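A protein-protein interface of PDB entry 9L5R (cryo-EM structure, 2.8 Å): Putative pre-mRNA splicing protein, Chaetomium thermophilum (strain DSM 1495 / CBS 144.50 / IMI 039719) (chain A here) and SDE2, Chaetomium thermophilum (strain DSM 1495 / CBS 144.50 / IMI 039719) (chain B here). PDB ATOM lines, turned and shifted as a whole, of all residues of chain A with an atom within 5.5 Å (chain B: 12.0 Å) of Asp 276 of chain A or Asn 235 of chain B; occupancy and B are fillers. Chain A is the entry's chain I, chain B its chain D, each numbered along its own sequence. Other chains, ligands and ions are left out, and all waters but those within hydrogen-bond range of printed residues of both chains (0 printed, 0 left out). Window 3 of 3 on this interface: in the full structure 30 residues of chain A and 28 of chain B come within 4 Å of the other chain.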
ATOM      1  N   ASN A 274      16.096 -12.716   5.276  1.00  0.00           N
ATOM      2  CA  ASN A 274      16.080 -12.857   3.819  1.00  0.00           C
ATOM      3  C   ASN A 274      16.553 -11.545   3.187  1.00  0.00           C
ATOM      4  O   ASN A 274      15.772 -10.711   2.722  1.00  0.00           O
ATOM      5  CB  ASN A 274      14.688 -13.252   3.347  1.00  0.00           C
ATOM      6  CG  ASN A 274      14.717 -14.268   2.225  1.00  0.00           C
ATOM      7  OD1 ASN A 274      15.776 -14.588   1.686  1.00  0.00           O
ATOM      8  ND2 ASN A 274      13.550 -14.797   1.877  1.00  0.00           N
ATOM      9  N   PHE A 275      17.879 -11.381   3.188  1.00  0.00           N
ATOM     10  CA  PHE A 275      18.486 -10.113   2.788  1.00  0.00           C
ATOM     11  C   PHE A 275      18.316  -9.849   1.296  1.00  0.00           C
ATOM     12  O   PHE A 275      18.078  -8.707   0.884  1.00  0.00           O
ATOM     13  CB  PHE A 275      19.969 -10.098   3.165  1.00  0.00           C
ATOM     14  CG  PHE A 275      20.237  -9.743   4.607  1.00  0.00           C
ATOM     15  CD1 PHE A 275      19.202  -9.646   5.527  1.00  0.00           C
ATOM     16  CD2 PHE A 275      21.533  -9.506   5.038  1.00  0.00           C
ATOM     17  CE1 PHE A 275      19.458  -9.321   6.848  1.00  0.00           C
ATOM     18  CE2 PHE A 275      21.794  -9.180   6.357  1.00  0.00           C
ATOM     19  CZ  PHE A 275      20.755  -9.088   7.262  1.00  0.00           C
ATOM     20  N   ASP A 276      18.440 -10.891   0.470  1.00  0.00           N
ATOM     21  CA  ASP A 276      18.305 -10.711  -0.973  1.00  0.00           C
ATOM     22  C   ASP A 276      16.874 -10.355  -1.364  1.00  0.00           C
ATOM     23  O   ASP A 276      16.657  -9.510  -2.240  1.00  0.00           O
ATOM     24  CB  ASP A 276      18.776 -11.969  -1.703  1.00  0.00           C
ATOM     25  CG  ASP A 276      18.223 -13.238  -1.092  1.00  0.00           C
ATOM     26  OD1 ASP A 276      17.562 -13.149  -0.038  1.00  0.00           O
ATOM     27  OD2 ASP A 276      18.447 -14.324  -1.667  1.00  0.00           O
ATOM     28  N   ARG A 277      15.881 -10.971  -0.716  1.00  0.00           N
ATOM     29  CA  ARG A 277      14.497 -10.599  -0.998  1.00  0.00           C
ATOM     30  C   ARG A 277      14.161  -9.230  -0.428  1.00  0.00           C
ATOM     31  O   ARG A 277      13.348  -8.501  -1.014  1.00  0.00           O
ATOM     32  CB  ARG A 277      13.541 -11.665  -0.462  1.00  0.00           C
ATOM     33  CG  ARG A 277      13.825 -13.072  -0.985  1.00  0.00           C
ATOM     34  CD  ARG A 277      13.390 -13.288  -2.444  1.00  0.00           C
ATOM     35  NE  ARG A 277      14.327 -12.730  -3.415  1.00  0.00           N
ATOM     36  CZ  ARG A 277      15.546 -13.196  -3.658  1.00  0.00           C
ATOM     37  NH1 ARG A 277      15.997 -14.295  -3.079  1.00  0.00           N
ATOM     38  NH2 ARG A 277      16.324 -12.549  -4.519  1.00  0.00           N
ATOM     39  N   ALA A 278      14.785  -8.863   0.696  1.00  0.00           N
ATOM     40  CA  ALA A 278      14.671  -7.499   1.199  1.00  0.00           C
ATOM     41  C   ALA A 278      15.195  -6.500   0.178  1.00  0.00           C
ATOM     42  O   ALA A 278      14.550  -5.482  -0.086  1.00  0.00           O
ATOM     43  CB  ALA A 278      15.429  -7.356   2.518  1.00  0.00           C
ATOM     44  N   ARG A 279      16.339  -6.805  -0.441  1.00  0.00           N
ATOM     45  CA  ARG A 279      16.898  -5.929  -1.468  1.00  0.00           C
ATOM     46  C   ARG A 279      16.020  -5.890  -2.716  1.00  0.00           C
ATOM     47  O   ARG A 279      15.887  -4.840  -3.353  1.00  0.00           O
ATOM     48  CB  ARG A 279      18.314  -6.379  -1.825  1.00  0.00           C
ATOM     49  CG  ARG A 279      19.368  -5.982  -0.805  1.00  0.00           C
ATOM     50  CD  ARG A 279      20.745  -6.464  -1.227  1.00  0.00           C
ATOM     51  NE  ARG A 279      21.782  -6.052  -0.289  1.00  0.00           N
ATOM     52  CZ  ARG A 279      22.140  -6.746   0.781  1.00  0.00           C
ATOM     53  NH1 ARG A 279      21.545  -7.886   1.096  1.00  0.00           N
ATOM     54  NH2 ARG A 279      23.116  -6.286   1.558  1.00  0.00           N
ATOM     55  N   ASP A 280      15.418  -7.026  -3.084  1.00  0.00           N
ATOM     56  CA  ASP A 280      14.565  -7.068  -4.272  1.00  0.00           C
ATOM     57  C   ASP A 280      13.310  -6.220  -4.092  1.00  0.00           C
ATOM     58  O   ASP A 280      12.997  -5.369  -4.936  1.00  0.00           O
ATOM     59  CB  ASP A 280      14.190  -8.514  -4.599  1.00  0.00           C
ATOM     60  CG  ASP A 280      15.272  -9.233  -5.375  1.00  0.00           C
ATOM     61  OD1 ASP A 280      16.008  -8.561  -6.126  1.00  0.00           O
ATOM     62  OD2 ASP A 280      15.386 -10.467  -5.237  1.00  0.00           O
ATOM     63  N   VAL A 281      12.588  -6.424  -2.984  1.00  0.00           N
ATOM     64  CA  VAL A 281      11.413  -5.603  -2.693  1.00  0.00           C
ATOM     65  C   VAL A 281      11.823  -4.156  -2.447  1.00  0.00           C
ATOM     66  O   VAL A 281      11.071  -3.221  -2.756  1.00  0.00           O
ATOM     67  CB  VAL A 281      10.636  -6.203  -1.502  1.00  0.00           C
ATOM     68  CG1 VAL A 281       9.353  -5.437  -1.240  1.00  0.00           C
ATOM     69  CG2 VAL A 281      10.308  -7.661  -1.774  1.00  0.00           C
ATOM     70  N   ARG A 337      30.043  -6.350  -2.480  1.00  0.00           N
ATOM     71  CA  ARG A 337      29.061  -5.568  -1.727  1.00  0.00           C
ATOM     72  C   ARG A 337      29.361  -4.080  -1.821  1.00  0.00           C
ATOM     73  O   ARG A 337      28.452  -3.269  -2.031  1.00  0.00           O
ATOM     74  CB  ARG A 337      29.022  -5.997  -0.261  1.00  0.00           C
ATOM     75  CG  ARG A 337      28.497  -7.390  -0.021  1.00  0.00           C
ATOM     76  CD  ARG A 337      28.464  -7.719   1.456  1.00  0.00           C
ATOM     77  NE  ARG A 337      28.055  -9.102   1.666  1.00  0.00           N
ATOM     78  CZ  ARG A 337      26.804  -9.514   1.799  1.00  0.00           C
ATOM     79  NH1 ARG A 337      25.788  -8.667   1.763  1.00  0.00           N
ATOM     80  NH2 ARG A 337      26.566 -10.811   1.960  1.00  0.00           N
ATOM     81  N   ARG A 340      28.426  -2.893  -5.251  1.00  0.00           N
ATOM     82  CA  ARG A 340      26.984  -2.678  -5.329  1.00  0.00           C
ATOM     83  C   ARG A 340      26.581  -1.383  -4.638  1.00  0.00           C
ATOM     84  O   ARG A 340      25.808  -0.591  -5.186  1.00  0.00           O
ATOM     85  CB  ARG A 340      26.241  -3.864  -4.712  1.00  0.00           C
ATOM     86  CG  ARG A 340      26.190  -5.112  -5.577  1.00  0.00           C
ATOM     87  CD  ARG A 340      25.945  -6.345  -4.721  1.00  0.00           C
ATOM     88  NE  ARG A 340      25.336  -7.434  -5.477  1.00  0.00           N
ATOM     89  CZ  ARG A 340      24.303  -8.150  -5.054  1.00  0.00           C
ATOM     90  NH1 ARG A 340      23.734  -7.917  -3.882  1.00  0.00           N
ATOM     91  NH2 ARG A 340      23.828  -9.123  -5.825  1.00  0.00           N
ATOM     92  N   ALA B 226      19.984  -9.849  14.073  1.00  0.00           N
ATOM     93  CA  ALA B 226      20.137 -10.736  12.926  1.00  0.00           C
ATOM     94  C   ALA B 226      21.493 -11.427  12.931  1.00  0.00           C
ATOM     95  O   ALA B 226      21.574 -12.643  12.719  1.00  0.00           O
ATOM     96  CB  ALA B 226      19.936  -9.955  11.627  1.00  0.00           C
ATOM     97  N   MET B 227      22.571 -10.679  13.178  1.00  0.00           N
ATOM     98  CA  MET B 227      23.852 -11.373  13.337  1.00  0.00           C
ATOM     99  C   MET B 227      24.129 -11.856  14.758  1.00  0.00           C
ATOM    100  O   MET B 227      25.188 -12.454  14.984  1.00  0.00           O
ATOM    101  CB  MET B 227      25.026 -10.538  12.828  1.00  0.00           C
ATOM    102  CG  MET B 227      25.139 -10.548  11.310  1.00  0.00           C
ATOM    103  SD  MET B 227      23.887  -9.578  10.488  1.00  0.00           S
ATOM    104  CE  MET B 227      24.549  -7.969  10.873  1.00  0.00           C
ATOM    105  N   ALA B 231      21.639 -14.802  10.918  1.00  0.00           N
ATOM    106  CA  ALA B 231      20.651 -14.735   9.848  1.00  0.00           C
ATOM    107  C   ALA B 231      21.299 -14.441   8.497  1.00  0.00           C
ATOM    108  O   ALA B 231      20.745 -13.716   7.670  1.00  0.00           O
ATOM    109  CB  ALA B 231      19.584 -13.692  10.166  1.00  0.00           C
ATOM    110  N   TRP B 232      22.483 -15.002   8.261  1.00  0.00           N
ATOM    111  CA  TRP B 232      23.196 -14.779   7.008  1.00  0.00           C
ATOM    112  C   TRP B 232      22.568 -15.622   5.904  1.00  0.00           C
ATOM    113  O   TRP B 232      22.816 -16.828   5.816  1.00  0.00           O
ATOM    114  CB  TRP B 232      24.675 -15.113   7.172  1.00  0.00           C
ATOM    115  CG  TRP B 232      25.515 -13.958   7.628  1.00  0.00           C
ATOM    116  CD1 TRP B 232      26.111 -13.810   8.847  1.00  0.00           C
ATOM    117  CD2 TRP B 232      25.858 -12.789   6.871  1.00  0.00           C
ATOM    118  NE1 TRP B 232      26.801 -12.623   8.897  1.00  0.00           N
ATOM    119  CE2 TRP B 232      26.661 -11.978   7.697  1.00  0.00           C
ATOM    120  CE3 TRP B 232      25.562 -12.351   5.576  1.00  0.00           C
ATOM    121  CZ2 TRP B 232      27.172 -10.753   7.271  1.00  0.00           C
ATOM    122  CZ3 TRP B 232      26.070 -11.134   5.157  1.00  0.00           C
ATOM    123  CH2 TRP B 232      26.866 -10.350   6.000  1.00  0.00           C
ATOM    124  N   LYS B 233      21.753 -14.987   5.058  1.00  0.00           N
ATOM    125  CA  LYS B 233      21.164 -15.653   3.902  1.00  0.00           C
ATOM    126  C   LYS B 233      21.271 -14.780   2.657  1.00  0.00           C
ATOM    127  O   LYS B 233      20.414 -14.848   1.768  1.00  0.00           O
ATOM    128  CB  LYS B 233      19.703 -16.028   4.162  1.00  0.00           C
ATOM    129  CG  LYS B 233      19.273 -17.346   3.531  1.00  0.00           C
ATOM    130  CD  LYS B 233      17.873 -17.738   3.968  1.00  0.00           C
ATOM    131  CE  LYS B 233      17.849 -18.141   5.432  1.00  0.00           C
ATOM    132  NZ  LYS B 233      18.653 -19.372   5.674  1.00  0.00           N
ATOM    133  N   ASP B 234      22.310 -13.957   2.580  1.00  0.00           N
ATOM    134  CA  ASP B 234      22.509 -13.078   1.442  1.00  0.00           C
ATOM    135  C   ASP B 234      23.018 -13.867   0.237  1.00  0.00           C
ATOM    136  O   ASP B 234      23.435 -15.023   0.343  1.00  0.00           O
ATOM    137  CB  ASP B 234      23.483 -11.959   1.800  1.00  0.00           C
ATOM    138  CG  ASP B 234      23.142 -10.649   1.122  1.00  0.00           C
ATOM    139  OD1 ASP B 234      22.725 -10.679  -0.055  1.00  0.00           O
ATOM    140  OD2 ASP B 234      23.292  -9.590   1.765  1.00  0.00           O
ATOM    141  N   ASN B 235      22.978 -13.222  -0.923  1.00  0.00           N
ATOM    142  CA  ASN B 235      23.377 -13.868  -2.165  1.00  0.00           C
ATOM    143  C   ASN B 235      24.134 -12.904  -3.074  1.00  0.00           C
ATOM    144  O   ASN B 235      23.705 -12.624  -4.194  1.00  0.00           O
ATOM    145  CB  ASN B 235      22.149 -14.421  -2.888  1.00  0.00           C
ATOM    146  CG  ASN B 235      21.827 -15.846  -2.488  1.00  0.00           C
ATOM    147  OD1 ASN B 235      22.712 -16.699  -2.424  1.00  0.00           O
ATOM    148  ND2 ASN B 235      20.554 -16.112  -2.218  1.00  0.00           N
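The guanidinium group of Arg 337 of chain A is in salt-bridge range of the side-chain carboxylate of Asp 234 of chain B (2.7 Å).
ND2 of Asn 235 of chain B is in hydrogen-bond range of OD2 of Asp 276 of chain A (2.8 Å).
OD2 of Asp 234 of chain B lies within salt-bridge range of NH1 of Arg 279 of chain A.
Among the printed residues, merely in contact across the chains: Phe 275 of chain A with Asp 234 of chain B, Asp 276 of chain A with Lys 233 of chain B, Arg 337 of chain A with Trp 232 of chain B and Arg 340 of chain A with Asn 235 of chain B.
Asn 235 of chain B touches just these residues of chain A: Asp 276 (2.8 Å) and Arg 340 (3.9 Å).
No residue of chain B comes within 4 Å of Asn 274 of chain A.
Phe 275 of chain A touches one residue of chain B.
No residue of chain B comes within 4 Å of Arg 277 of chain A.
No residue of chain B comes within 4 Å of Ala 278 of chain A.
Of chain B, only Asp 234 (2.5 Å) comes within 4 Å of Arg 279 of chain A.
Of the printed residues of chain A, Trp 232 of chain B touches Arg 337.
Of the printed residues of chain B, Arg 337 of chain A touches Trp 232 (3.3 Å) and Asp 234 (2.7 Å).
Val 281 of chain A touches none of the printed residues of chain B.
The nearest residue of chain A that does not touch Asn 235 of chain B is Arg 277 of chain A (5.0 Å).
The nearest printed residue of chain A that does not touch Lys 233 of chain B is Asn 274 of chain A (4.4 Å).
Hydrophobic or aromatic side chains of chain B within 4 Å of the printed part of chain A: Trp 232.
Hydrophobic or aromatic side chains of chain A that line the printed part of chain B: Phe 275.
OD1 of Asp 276 of chain A sits close to OD1 of Asn 274 of chain A.
The side-chain carboxylate (OD2) of Asp 276 of chain A lies within salt-bridge range of the guanidinium group (NH1) of Arg 277 of chain A, at 2.8 Å.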
